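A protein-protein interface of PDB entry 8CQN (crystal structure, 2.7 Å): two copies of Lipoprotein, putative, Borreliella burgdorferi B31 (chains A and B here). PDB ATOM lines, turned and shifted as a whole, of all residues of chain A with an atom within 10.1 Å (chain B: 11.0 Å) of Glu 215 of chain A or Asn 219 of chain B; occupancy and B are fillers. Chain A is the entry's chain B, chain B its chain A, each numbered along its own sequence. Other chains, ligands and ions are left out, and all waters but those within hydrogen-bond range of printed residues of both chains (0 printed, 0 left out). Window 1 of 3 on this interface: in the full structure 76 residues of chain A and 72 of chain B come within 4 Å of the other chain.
OD1 of Asn 219 of chain A lies within hydrogen-bond range of NZ of Lys 212 of chain B.
OD1 of Asn 219 of chain B lies within hydrogen-bond range of ND2 of Asn 219 of chain A (2.6 Å).
Glu 215 of chain A touches one residue of chain B.
Ser 216 of chain A touches just these residues of chain B: Ser 216, Asn 219 and Arg 220.
Of chain B, only Lys 212 (3.4 Å), Glu 215 (3.7 Å), Ser 216 (3.6 Å) and Asn 219 (2.6 Å) come within 4 Å of Asn 219 of chain A.
No residue of chain A comes within 4 Å of Asn 218 of chain B.
Of the printed residues of chain A, Ala 223 of chain B touches Ser 209 and Arg 213.
Of the printed residues of chain B, Glu 208 of chain A touches Leu 226 (3.7 Å).
Of the printed residues of chain A, Ser 227 of chain B touches Glu 95 (3.99 Å) and Ser 209 (3.6 Å).
Of the printed residues of chain A, Arg 220 of chain B touches Ser 216.
Of the printed residues of chain A, Tyr 222 of chain B touches Lys 212 (3.9 Å).
Lys 217 of chain B touches none of the printed residues of chain A.
Lys 225 of chain B touches none of the printed residues of chain A.
The nearest residue of chain B that does not touch Glu 215 of chain A is Glu 215 of chain B (4.3 Å).
The nearest residue of chain A that does not touch Asn 219 of chain B is Arg 213 of chain A (5.1 Å).
Along chain B the printed residues that touch a printed residue of chain A span positions 212 to 227.
Of the 18 printed residues of chain A, 10 touch a printed residue of chain B.
Printed residues of chain A that touch a printed residue of chain B: Glu 95, Glu 208, Ser 209, Lys 212, Arg 213, Glu 215, Ser 216, Asn 219, Arg 220 and Ala 223.
Hydrophobic or aromatic side chains of chain A that line the printed part of chain B: Ala 223.
OG of Ser 227 of chain B sits at hydrogen-bond distance from O of Ala 223 of chain B (3.5 Å).
The backbone carbonyl oxygen (O) of Glu 215 of chain B lies close to the side-chain amide oxygen (OD1) of Asn 219 of chain B (3.3 Å).
The side-chain amide nitrogen (ND2) of Asn 219 of chain A lies within hydrogen-bond range of the backbone carbonyl oxygen (O) of Glu 215 of chain A (3.3 Å).
OE2 of Glu 95 of chain A lies within salt-bridge range of NE of Arg 213 of chain A (2.8 Å).
Among the printed residues, merely in contact across the chains: Ser 216 of chain A with Ser 216 of chain B (2.9 Å), Ser 209 of chain A with Ala 223 of chain B (3.1 Å), Ser 209 of chain A with Leu 226 of chain B (3.4 Å), Lys 212 of chain A with Asn 219 of chain B (3.5 Å), Glu 215 of chain A with Asn 219 of chain B (3.5 Å), Ser 209 of chain A with Ser 227 of chain B (3.6 Å), Ser 216 of chain A with Arg 220 of chain B (3.6 Å), Asn 219 of chain A with Ser 216 of chain B (3.6 Å), Asn 219 of chain A with Glu 215 of chain B (3.7 Å), Glu 208 of chain A with Leu 226 of chain B (3.7 Å), Ser 216 of chain A with Asn 219 of chain B (3.7 Å), Ala 223 of chain A with Lys 212 of chain B (3.8 Å), Lys 212 of chain A with Tyr 222 of chain B (3.9 Å), Arg 213 of chain A with Ala 223 of chain B (3.9 Å), Ala 223 of chain A with Arg 213 of chain B (3.9 Å), Arg 220 of chain A with Ser 216 of chain B (3.9 Å) and Glu 95 of chain A with Ser 227 of chain B (3.99 Å).
Lys 212 of chain A touches Asn 219 of chain B, and with the chains exchanged Asn 219 of chain A touches Lys 212 of chain B.
Glu 215 of chain A touches Asn 219 of chain B, and with the chains exchanged Asn 219 of chain A touches Glu 215 of chain B.
Ala 223 of chain A touches Lys 212 of chain B, but with the chains exchanged Lys 212 of chain A does not touch Ala 223 of chain B (4.01 Å).
Positions printed for both chains: 210, 211, 212, 213, 214, 215, 216, 217, 218, 219, 220, 221, 222 and 223.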
ATOM      1  N   GLU A  95       2.606   3.369  26.376  1.00  0.00           N
ATOM      2  CA  GLU A  95       2.646   2.661  27.678  1.00  0.00           C
ATOM      3  C   GLU A  95       4.105   2.483  28.086  1.00  0.00           C
ATOM      4  O   GLU A  95       4.464   2.798  29.232  1.00  0.00           O
ATOM      5  CB  GLU A  95       1.941   1.323  27.572  1.00  0.00           C
ATOM      6  CG  GLU A  95       0.444   1.454  27.420  1.00  0.00           C
ATOM      7  CD  GLU A  95      -0.254   0.225  26.852  1.00  0.00           C
ATOM      8  OE1 GLU A  95       0.454  -0.806  26.529  1.00  0.00           O
ATOM      9  OE2 GLU A  95      -1.513   0.306  26.700  1.00  0.00           O
ATOM     10  N   LYS A 207      -2.042   2.256  34.553  1.00  0.00           N
ATOM     11  CA  LYS A 207      -2.753   0.975  34.781  1.00  0.00           C
ATOM     12  C   LYS A 207      -4.082   1.076  34.024  1.00  0.00           C
ATOM     13  O   LYS A 207      -4.374   0.186  33.227  1.00  0.00           O
ATOM     14  CB  LYS A 207      -2.925   0.760  36.285  1.00  0.00           C
ATOM     15  CG  LYS A 207      -2.524  -0.594  36.834  1.00  0.00           C
ATOM     16  CD  LYS A 207      -1.916  -0.487  38.222  1.00  0.00           C
ATOM     17  CE  LYS A 207      -0.461  -0.046  38.165  1.00  0.00           C
ATOM     18  NZ  LYS A 207       0.228  -0.257  39.459  1.00  0.00           N
ATOM     19  N   GLU A 208      -4.843   2.144  34.266  1.00  0.00           N
ATOM     20  CA  GLU A 208      -6.063   2.478  33.485  1.00  0.00           C
ATOM     21  C   GLU A 208      -5.776   2.254  31.978  1.00  0.00           C
ATOM     22  O   GLU A 208      -6.601   1.535  31.322  1.00  0.00           O
ATOM     23  CB  GLU A 208      -6.542   3.888  33.852  1.00  0.00           C
ATOM     24  CG  GLU A 208      -7.341   3.970  35.157  1.00  0.00           C
ATOM     25  CD  GLU A 208      -7.178   5.200  36.053  1.00  0.00           C
ATOM     26  OE1 GLU A 208      -7.237   5.044  37.307  1.00  0.00           O
ATOM     27  OE2 GLU A 208      -6.989   6.319  35.521  1.00  0.00           O
ATOM     28  N   SER A 209      -4.673   2.766  31.401  1.00  0.00           N
ATOM     29  CA  SER A 209      -4.533   2.730  29.912  1.00  0.00           C
ATOM     30  C   SER A 209      -4.437   1.279  29.445  1.00  0.00           C
ATOM     31  O   SER A 209      -5.132   0.904  28.485  1.00  0.00           O
ATOM     32  CB  SER A 209      -3.407   3.559  29.356  1.00  0.00           C
ATOM     33  OG  SER A 209      -2.166   3.083  29.785  1.00  0.00           O
ATOM     34  N   ILE A 210      -3.628   0.482  30.132  1.00  0.00           N
ATOM     35  CA  ILE A 210      -3.392  -0.943  29.758  1.00  0.00           C
ATOM     36  C   ILE A 210      -4.754  -1.638  29.803  1.00  0.00           C
ATOM     37  O   ILE A 210      -5.146  -2.313  28.834  1.00  0.00           O
ATOM     38  CB  ILE A 210      -2.347  -1.584  30.699  1.00  0.00           C
ATOM     39  CG1 ILE A 210      -0.964  -0.987  30.463  1.00  0.00           C
ATOM     40  CG2 ILE A 210      -2.298  -3.097  30.559  1.00  0.00           C
ATOM     41  CD1 ILE A 210      -0.011  -1.153  31.622  1.00  0.00           C
ATOM     42  N   ILE A 211      -5.469  -1.441  30.899  1.00  0.00           N
ATOM     43  CA  ILE A 211      -6.795  -2.067  31.132  1.00  0.00           C
ATOM     44  C   ILE A 211      -7.729  -1.570  30.037  1.00  0.00           C
ATOM     45  O   ILE A 211      -8.363  -2.343  29.394  1.00  0.00           O
ATOM     46  CB  ILE A 211      -7.306  -1.740  32.548  1.00  0.00           C
ATOM     47  CG1 ILE A 211      -6.724  -2.738  33.545  1.00  0.00           C
ATOM     48  CG2 ILE A 211      -8.829  -1.742  32.621  1.00  0.00           C
ATOM     49  CD1 ILE A 211      -6.767  -2.258  34.968  1.00  0.00           C
ATOM     50  N   LYS A 212      -7.748  -0.288  29.804  1.00  0.00           N
ATOM     51  CA  LYS A 212      -8.639   0.266  28.788  1.00  0.00           C
ATOM     52  C   LYS A 212      -8.278  -0.308  27.432  1.00  0.00           C
ATOM     53  O   LYS A 212      -9.175  -0.415  26.600  1.00  0.00           O
ATOM     54  CB  LYS A 212      -8.475   1.777  28.772  1.00  0.00           C
ATOM     55  CG  LYS A 212      -9.780   2.482  28.542  1.00  0.00           C
ATOM     56  CD  LYS A 212     -10.687   2.325  29.738  1.00  0.00           C
ATOM     57  CE  LYS A 212     -12.144   2.395  29.322  1.00  0.00           C
ATOM     58  NZ  LYS A 212     -13.060   1.786  30.310  1.00  0.00           N
ATOM     59  N   ARG A 213      -7.001  -0.584  27.180  1.00  0.00           N
ATOM     60  CA  ARG A 213      -6.590  -1.046  25.830  1.00  0.00           C
ATOM     61  C   ARG A 213      -7.170  -2.431  25.628  1.00  0.00           C
ATOM     62  O   ARG A 213      -7.748  -2.682  24.553  1.00  0.00           O
ATOM     63  CB  ARG A 213      -5.078  -1.106  25.672  1.00  0.00           C
ATOM     64  CG  ARG A 213      -4.654  -1.950  24.492  1.00  0.00           C
ATOM     65  CD  ARG A 213      -3.256  -1.553  24.113  1.00  0.00           C
ATOM     66  NE  ARG A 213      -2.342  -1.928  25.175  1.00  0.00           N
ATOM     67  CZ  ARG A 213      -2.014  -3.177  25.479  1.00  0.00           C
ATOM     68  NH1 ARG A 213      -2.504  -4.193  24.790  1.00  0.00           N
ATOM     69  NH2 ARG A 213      -1.178  -3.413  26.470  1.00  0.00           N
ATOM     70  N   LEU A 214      -7.032  -3.267  26.657  1.00  0.00           N
ATOM     71  CA  LEU A 214      -7.561  -4.645  26.619  1.00  0.00           C
ATOM     72  C   LEU A 214      -9.081  -4.579  26.493  1.00  0.00           C
ATOM     73  O   LEU A 214      -9.631  -5.382  25.734  1.00  0.00           O
ATOM     74  CB  LEU A 214      -7.135  -5.397  27.878  1.00  0.00           C
ATOM     75  CG  LEU A 214      -5.623  -5.554  28.045  1.00  0.00           C
ATOM     76  CD1 LEU A 214      -5.274  -6.349  29.295  1.00  0.00           C
ATOM     77  CD2 LEU A 214      -4.986  -6.190  26.821  1.00  0.00           C
ATOM     78  N   GLU A 215      -9.726  -3.650  27.191  1.00  0.00           N
ATOM     79  CA  GLU A 215     -11.204  -3.499  27.140  1.00  0.00           C
ATOM     80  C   GLU A 215     -11.604  -3.189  25.695  1.00  0.00           C
ATOM     81  O   GLU A 215     -12.624  -3.709  25.208  1.00  0.00           O
ATOM     82  CB  GLU A 215     -11.697  -2.425  28.109  1.00  0.00           C
ATOM     83  CG  GLU A 215     -13.216  -2.361  28.220  1.00  0.00           C
ATOM     84  CD  GLU A 215     -13.787  -1.179  29.014  1.00  0.00           C
ATOM     85  OE1 GLU A 215     -12.994  -0.530  29.777  1.00  0.00           O
ATOM     86  OE2 GLU A 215     -15.025  -0.895  28.877  1.00  0.00           O
ATOM     87  N   SER A 216     -10.818  -2.387  25.004  1.00  0.00           N
ATOM     88  CA  SER A 216     -11.201  -1.958  23.641  1.00  0.00           C
ATOM     89  C   SER A 216     -11.196  -3.184  22.742  1.00  0.00           C
ATOM     90  O   SER A 216     -12.011  -3.222  21.838  1.00  0.00           O
ATOM     91  CB  SER A 216     -10.311  -0.901  23.123  1.00  0.00           C
ATOM     92  OG  SER A 216      -9.567  -1.407  22.044  1.00  0.00           O
ATOM     93  N   LYS A 217     -10.338  -4.161  23.004  1.00  0.00           N
ATOM     94  CA  LYS A 217     -10.212  -5.341  22.102  1.00  0.00           C
ATOM     95  C   LYS A 217     -11.389  -6.321  22.323  1.00  0.00           C
ATOM     96  O   LYS A 217     -11.841  -6.924  21.314  1.00  0.00           O
ATOM     97  CB  LYS A 217      -8.816  -5.963  22.240  1.00  0.00           C
ATOM     98  CG  LYS A 217      -8.753  -7.351  22.849  1.00  0.00           C
ATOM     99  CD  LYS A 217      -7.373  -8.004  22.764  1.00  0.00           C
ATOM    100  CE  LYS A 217      -7.095  -8.860  23.990  1.00  0.00           C
ATOM    101  NZ  LYS A 217      -5.954  -9.780  23.790  1.00  0.00           N
ATOM    102  N   ASN A 218     -11.880  -6.453  23.563  1.00  0.00           N
ATOM    103  CA  ASN A 218     -13.018  -7.317  23.946  1.00  0.00           C
ATOM    104  C   ASN A 218     -14.292  -6.758  23.331  1.00  0.00           C
ATOM    105  O   ASN A 218     -15.043  -7.527  22.683  1.00  0.00           O
ATOM    106  CB  ASN A 218     -13.231  -7.394  25.456  1.00  0.00           C
ATOM    107  CG  ASN A 218     -12.115  -8.117  26.178  1.00  0.00           C
ATOM    108  OD1 ASN A 218     -11.422  -8.944  25.590  1.00  0.00           O
ATOM    109  ND2 ASN A 218     -11.912  -7.777  27.440  1.00  0.00           N
ATOM    110  N   ASN A 219     -14.517  -5.468  23.554  1.00  0.00           N
ATOM    111  CA  ASN A 219     -15.567  -4.684  22.865  1.00  0.00           C
ATOM    112  C   ASN A 219     -15.499  -4.949  21.363  1.00  0.00           C
ATOM    113  O   ASN A 219     -16.564  -4.966  20.740  1.00  0.00           O
ATOM    114  CB  ASN A 219     -15.396  -3.195  23.108  1.00  0.00           C
ATOM    115  CG  ASN A 219     -15.786  -2.796  24.510  1.00  0.00           C
ATOM    116  OD1 ASN A 219     -16.577  -3.481  25.159  1.00  0.00           O
ATOM    117  ND2 ASN A 219     -15.263  -1.664  24.955  1.00  0.00           N
ATOM    118  N   ARG A 220     -14.305  -5.115  20.787  1.00  0.00           N
ATOM    119  CA  ARG A 220     -14.234  -5.298  19.321  1.00  0.00           C
ATOM    120  C   ARG A 220     -14.614  -6.740  19.014  1.00  0.00           C
ATOM    121  O   ARG A 220     -15.298  -6.977  18.037  1.00  0.00           O
ATOM    122  CB  ARG A 220     -12.869  -4.926  18.745  1.00  0.00           C
ATOM    123  CG  ARG A 220     -12.875  -4.789  17.229  1.00  0.00           C
ATOM    124  CD  ARG A 220     -11.512  -4.423  16.675  1.00  0.00           C
ATOM    125  NE  ARG A 220     -10.508  -5.454  16.948  1.00  0.00           N
ATOM    126  CZ  ARG A 220      -9.186  -5.256  17.031  1.00  0.00           C
ATOM    127  NH1 ARG A 220      -8.678  -4.044  16.866  1.00  0.00           N
ATOM    128  NH2 ARG A 220      -8.376  -6.279  17.284  1.00  0.00           N
ATOM    129  N   SER A 221     -14.172  -7.678  19.828  1.00  0.00           N
ATOM    130  CA  SER A 221     -14.558  -9.100  19.693  1.00  0.00           C
ATOM    131  C   SER A 221     -16.085  -9.254  19.690  1.00  0.00           C
ATOM    132  O   SER A 221     -16.613 -10.103  18.927  1.00  0.00           O
ATOM    133  CB  SER A 221     -13.969  -9.901  20.790  1.00  0.00           C
ATOM    134  OG  SER A 221     -12.940 -10.690  20.259  1.00  0.00           O
ATOM    135  N   TYR A 222     -16.751  -8.514  20.573  1.00  0.00           N
ATOM    136  CA  TYR A 222     -18.211  -8.585  20.791  1.00  0.00           C
ATOM    137  C   TYR A 222     -18.897  -7.906  19.608  1.00  0.00           C
ATOM    138  O   TYR A 222     -19.999  -8.287  19.259  1.00  0.00           O
ATOM    139  CB  TYR A 222     -18.570  -7.993  22.159  1.00  0.00           C
ATOM    140  CG  TYR A 222     -19.902  -8.448  22.708  1.00  0.00           C
ATOM    141  CD1 TYR A 222     -20.012  -9.599  23.474  1.00  0.00           C
ATOM    142  CD2 TYR A 222     -21.064  -7.729  22.454  1.00  0.00           C
ATOM    143  CE1 TYR A 222     -21.239 -10.023  23.965  1.00  0.00           C
ATOM    144  CE2 TYR A 222     -22.293  -8.133  22.943  1.00  0.00           C
ATOM    145  CZ  TYR A 222     -22.380  -9.286  23.695  1.00  0.00           C
ATOM    146  OH  TYR A 222     -23.584  -9.680  24.180  1.00  0.00           O
ATOM    147  N   ALA A 223     -18.246  -6.930  18.997  1.00  0.00           N
ATOM    148  CA  ALA A 223     -18.805  -6.166  17.867  1.00  0.00           C
ATOM    149  C   ALA A 223     -18.846  -7.085  16.647  1.00  0.00           C
ATOM    150  O   ALA A 223     -19.829  -7.053  15.900  1.00  0.00           O
ATOM    151  CB  ALA A 223     -17.980  -4.937  17.629  1.00  0.00           C
ATOM    152  N   ILE B 210     -22.343  -1.927  15.396  1.00  0.00           N
ATOM    153  CA  ILE B 210     -21.756  -0.605  15.035  1.00  0.00           C
ATOM    154  C   ILE B 210     -21.526   0.211  16.316  1.00  0.00           C
ATOM    155  O   ILE B 210     -20.475   0.858  16.420  1.00  0.00           O
ATOM    156  CB  ILE B 210     -22.674   0.126  14.053  1.00  0.00           C
ATOM    157  CG1 ILE B 210     -22.845  -0.680  12.768  1.00  0.00           C
ATOM    158  CG2 ILE B 210     -22.184   1.544  13.776  1.00  0.00           C
ATOM    159  CD1 ILE B 210     -23.966  -0.172  11.872  1.00  0.00           C
ATOM    160  N   ILE B 211     -22.476   0.183  17.250  1.00  0.00           N
ATOM    161  CA  ILE B 211     -22.405   0.949  18.523  1.00  0.00           C
ATOM    162  C   ILE B 211     -21.225   0.384  19.305  1.00  0.00           C
ATOM    163  O   ILE B 211     -20.494   1.192  19.869  1.00  0.00           O
ATOM    164  CB  ILE B 211     -23.737   0.899  19.312  1.00  0.00           C
ATOM    165  CG1 ILE B 211     -24.696   2.030  18.929  1.00  0.00           C
ATOM    166  CG2 ILE B 211     -23.484   0.918  20.810  1.00  0.00           C
ATOM    167  CD1 ILE B 211     -24.724   2.363  17.455  1.00  0.00           C
ATOM    168  N   LYS B 212     -21.042  -0.935  19.351  1.00  0.00           N
ATOM    169  CA  LYS B 212     -19.903  -1.524  20.121  1.00  0.00           C
ATOM    170  C   LYS B 212     -18.600  -1.160  19.411  1.00  0.00           C
ATOM    171  O   LYS B 212     -17.579  -0.990  20.096  1.00  0.00           O
ATOM    172  CB  LYS B 212     -19.916  -3.052  20.231  1.00  0.00           C
ATOM    173  CG  LYS B 212     -20.604  -3.603  21.452  1.00  0.00           C
ATOM    174  CD  LYS B 212     -19.828  -3.533  22.729  1.00  0.00           C
ATOM    175  CE  LYS B 212     -20.746  -3.387  23.931  1.00  0.00           C
ATOM    176  NZ  LYS B 212     -20.009  -3.749  25.157  1.00  0.00           N
ATOM    177  N   ARG B 213     -18.615  -1.131  18.081  1.00  0.00           N
ATOM    178  CA  ARG B 213     -17.374  -0.806  17.353  1.00  0.00           C
ATOM    179  C   ARG B 213     -16.951   0.552  17.897  1.00  0.00           C
ATOM    180  O   ARG B 213     -15.795   0.662  18.333  1.00  0.00           O
ATOM    181  CB  ARG B 213     -17.481  -0.814  15.824  1.00  0.00           C
ATOM    182  CG  ARG B 213     -16.182  -0.372  15.161  1.00  0.00           C
ATOM    183  CD  ARG B 213     -16.025  -0.561  13.649  1.00  0.00           C
ATOM    184  NE  ARG B 213     -17.176  -0.082  12.897  1.00  0.00           N
ATOM    185  CZ  ARG B 213     -17.593   1.181  12.794  1.00  0.00           C
ATOM    186  NH1 ARG B 213     -16.959   2.161  13.402  1.00  0.00           N
ATOM    187  NH2 ARG B 213     -18.680   1.455  12.101  1.00  0.00           N
ATOM    188  N   LEU B 214     -17.886   1.493  17.978  1.00  0.00           N
ATOM    189  CA  LEU B 214     -17.564   2.878  18.401  1.00  0.00           C
ATOM    190  C   LEU B 214     -17.097   2.870  19.861  1.00  0.00           C
ATOM    191  O   LEU B 214     -16.251   3.712  20.214  1.00  0.00           O
ATOM    192  CB  LEU B 214     -18.770   3.785  18.168  1.00  0.00           C
ATOM    193  CG  LEU B 214     -19.157   3.950  16.691  1.00  0.00           C
ATOM    194  CD1 LEU B 214     -20.496   4.664  16.542  1.00  0.00           C
ATOM    195  CD2 LEU B 214     -18.086   4.694  15.903  1.00  0.00           C
ATOM    196  N   GLU B 215     -17.615   1.952  20.677  1.00  0.00           N
ATOM    197  CA  GLU B 215     -17.234   1.813  22.098  1.00  0.00           C
ATOM    198  C   GLU B 215     -15.755   1.386  22.143  1.00  0.00           C
ATOM    199  O   GLU B 215     -14.968   2.052  22.841  1.00  0.00           O
ATOM    200  CB  GLU B 215     -18.180   0.852  22.814  1.00  0.00           C
ATOM    201  CG  GLU B 215     -18.303   1.117  24.314  1.00  0.00           C
ATOM    202  CD  GLU B 215     -18.898   0.007  25.181  1.00  0.00           C
ATOM    203  OE1 GLU B 215     -19.900  -0.620  24.748  1.00  0.00           O
ATOM    204  OE2 GLU B 215     -18.356  -0.237  26.304  1.00  0.00           O
ATOM    205  N   SER B 216     -15.336   0.359  21.402  1.00  0.00           N
ATOM    206  CA  SER B 216     -13.893  -0.009  21.361  1.00  0.00           C
ATOM    207  C   SER B 216     -13.026   1.160  20.813  1.00  0.00           C
ATOM    208  O   SER B 216     -11.886   1.379  21.307  1.00  0.00           O
ATOM    209  CB  SER B 216     -13.703  -1.228  20.569  1.00  0.00           C
ATOM    210  OG  SER B 216     -14.079  -0.930  19.244  1.00  0.00           O
ATOM    211  N   LYS B 217     -13.519   1.889  19.815  1.00  0.00           N
ATOM    212  CA  LYS B 217     -12.762   3.001  19.187  1.00  0.00           C
ATOM    213  C   LYS B 217     -12.504   4.041  20.290  1.00  0.00           C
ATOM    214  O   LYS B 217     -11.323   4.372  20.559  1.00  0.00           O
ATOM    215  CB  LYS B 217     -13.540   3.496  17.969  1.00  0.00           C
ATOM    216  CG  LYS B 217     -13.079   4.830  17.391  1.00  0.00           C
ATOM    217  CD  LYS B 217     -13.215   4.875  15.874  1.00  0.00           C
ATOM    218  CE  LYS B 217     -13.215   6.298  15.345  1.00  0.00           C
ATOM    219  NZ  LYS B 217     -12.658   6.378  13.966  1.00  0.00           N
ATOM    220  N   ASN B 218     -13.564   4.438  20.987  1.00  0.00           N
ATOM    221  CA  ASN B 218     -13.511   5.423  22.092  1.00  0.00           C
ATOM    222  C   ASN B 218     -12.604   4.908  23.213  1.00  0.00           C
ATOM    223  O   ASN B 218     -11.834   5.693  23.780  1.00  0.00           O
ATOM    224  CB  ASN B 218     -14.921   5.746  22.575  1.00  0.00           C
ATOM    225  CG  ASN B 218     -15.726   6.430  21.491  1.00  0.00           C
ATOM    226  OD1 ASN B 218     -15.150   7.005  20.580  1.00  0.00           O
ATOM    227  ND2 ASN B 218     -17.050   6.324  21.533  1.00  0.00           N
ATOM    228  N   ASN B 219     -12.708   3.628  23.517  1.00  0.00           N
ATOM    229  CA  ASN B 219     -11.931   2.964  24.584  1.00  0.00           C
ATOM    230  C   ASN B 219     -10.463   2.991  24.194  1.00  0.00           C
ATOM    231  O   ASN B 219      -9.682   3.258  25.080  1.00  0.00           O
ATOM    232  CB  ASN B 219     -12.472   1.565  24.875  1.00  0.00           C
ATOM    233  CG  ASN B 219     -13.737   1.668  25.710  1.00  0.00           C
ATOM    234  OD1 ASN B 219     -14.551   0.734  25.787  1.00  0.00           O
ATOM    235  ND2 ASN B 219     -13.916   2.829  26.337  1.00  0.00           N
ATOM    236  N   ARG B 220     -10.116   2.703  22.938  1.00  0.00           N
ATOM    237  CA  ARG B 220      -8.698   2.594  22.499  1.00  0.00           C
ATOM    238  C   ARG B 220      -8.075   3.991  22.486  1.00  0.00           C
ATOM    239  O   ARG B 220      -6.921   4.144  22.892  1.00  0.00           O
ATOM    240  CB  ARG B 220      -8.600   2.014  21.090  1.00  0.00           C
ATOM    241  CG  ARG B 220      -7.173   1.820  20.586  1.00  0.00           C
ATOM    242  CD  ARG B 220      -6.442   0.720  21.361  1.00  0.00           C
ATOM    243  NE  ARG B 220      -5.098   0.424  20.882  1.00  0.00           N
ATOM    244  CZ  ARG B 220      -4.007   1.124  21.196  1.00  0.00           C
ATOM    245  NH1 ARG B 220      -4.076   2.166  22.020  1.00  0.00           N
ATOM    246  NH2 ARG B 220      -2.840   0.761  20.681  1.00  0.00           N
ATOM    247  N   SER B 221      -8.842   4.959  21.990  1.00  0.00           N
ATOM    248  CA  SER B 221      -8.527   6.399  22.001  1.00  0.00           C
ATOM    249  C   SER B 221      -8.256   6.900  23.436  1.00  0.00           C
ATOM    250  O   SER B 221      -7.236   7.643  23.642  1.00  0.00           O
ATOM    251  CB  SER B 221      -9.649   7.086  21.341  1.00  0.00           C
ATOM    252  OG  SER B 221      -9.491   8.472  21.477  1.00  0.00           O
ATOM    253  N   TYR B 222      -9.055   6.475  24.418  1.00  0.00           N
ATOM    254  CA  TYR B 222      -8.919   6.875  25.851  1.00  0.00           C
ATOM    255  C   TYR B 222      -7.693   6.186  26.494  1.00  0.00           C
ATOM    256  O   TYR B 222      -6.942   6.794  27.303  1.00  0.00           O
ATOM    257  CB  TYR B 222     -10.203   6.526  26.600  1.00  0.00           C
ATOM    258  CG  TYR B 222     -10.322   7.082  27.996  1.00  0.00           C
ATOM    259  CD1 TYR B 222     -10.314   8.449  28.249  1.00  0.00           C
ATOM    260  CD2 TYR B 222     -10.527   6.238  29.071  1.00  0.00           C
ATOM    261  CE1 TYR B 222     -10.444   8.958  29.536  1.00  0.00           C
ATOM    262  CE2 TYR B 222     -10.685   6.730  30.357  1.00  0.00           C
ATOM    263  CZ  TYR B 222     -10.650   8.090  30.592  1.00  0.00           C
ATOM    264  OH  TYR B 222     -10.791   8.522  31.876  1.00  0.00           O
ATOM    265  N   ALA B 223      -7.438   4.940  26.117  1.00  0.00           N
ATOM    266  CA  ALA B 223      -6.178   4.242  26.451  1.00  0.00           C
ATOM    267  C   ALA B 223      -4.988   5.147  26.082  1.00  0.00           C
ATOM    268  O   ALA B 223      -4.151   5.488  26.988  1.00  0.00           O
ATOM    269  CB  ALA B 223      -6.106   2.904  25.743  1.00  0.00           C
ATOM    270  N   LEU B 224      -4.888   5.530  24.805  1.00  0.00           N
ATOM    271  CA  LEU B 224      -3.722   6.309  24.351  1.00  0.00           C
ATOM    272  C   LEU B 224      -3.635   7.525  25.277  1.00  0.00           C
ATOM    273  O   LEU B 224      -2.576   7.820  25.840  1.00  0.00           O
ATOM    274  CB  LEU B 224      -3.928   6.718  22.894  1.00  0.00           C
ATOM    275  CG  LEU B 224      -2.910   7.727  22.372  1.00  0.00           C
ATOM    276  CD1 LEU B 224      -1.505   7.171  22.448  1.00  0.00           C
ATOM    277  CD2 LEU B 224      -3.240   8.142  20.956  1.00  0.00           C
ATOM    278  N   LYS B 225      -4.744   8.221  25.436  1.00  0.00           N
ATOM    279  CA  LYS B 225      -4.702   9.514  26.149  1.00  0.00           C
ATOM    280  C   LYS B 225      -4.279   9.241  27.591  1.00  0.00           C
ATOM    281  O   LYS B 225      -3.488  10.040  28.121  1.00  0.00           O
ATOM    282  CB  LYS B 225      -6.064  10.172  25.970  1.00  0.00           C
ATOM    283  CG  LYS B 225      -6.408  11.235  26.970  1.00  0.00           C
ATOM    284  CD  LYS B 225      -7.872  11.624  26.907  1.00  0.00           C
ATOM    285  CE  LYS B 225      -8.201  12.724  27.901  1.00  0.00           C
ATOM    286  NZ  LYS B 225      -9.031  13.772  27.261  1.00  0.00           N
ATOM    287  N   LEU B 226      -4.820   8.186  28.213  1.00  0.00           N
ATOM    288  CA  LEU B 226      -4.378   7.739  29.561  1.00  0.00           C
ATOM    289  C   LEU B 226      -2.842   7.571  29.535  1.00  0.00           C
ATOM    290  O   LEU B 226      -2.123   8.143  30.408  1.00  0.00           O
ATOM    291  CB  LEU B 226      -5.143   6.470  29.979  1.00  0.00           C
ATOM    292  CG  LEU B 226      -6.614   6.666  30.409  1.00  0.00           C
ATOM    293  CD1 LEU B 226      -7.351   5.351  30.571  1.00  0.00           C
ATOM    294  CD2 LEU B 226      -6.739   7.448  31.701  1.00  0.00           C
ATOM    295  N   SER B 227      -2.309   6.896  28.531  1.00  0.00           N
ATOM    296  CA  SER B 227      -0.855   6.598  28.469  1.00  0.00           C
ATOM    297  C   SER B 227      -0.066   7.904  28.410  1.00  0.00           C
ATOM    298  O   SER B 227       1.024   7.946  29.047  1.00  0.00           O
ATOM    299  CB  SER B 227      -0.503   5.674  27.342  1.00  0.00           C
ATOM    300  OG  SER B 227      -0.869   6.223  26.106  1.00  0.00           O
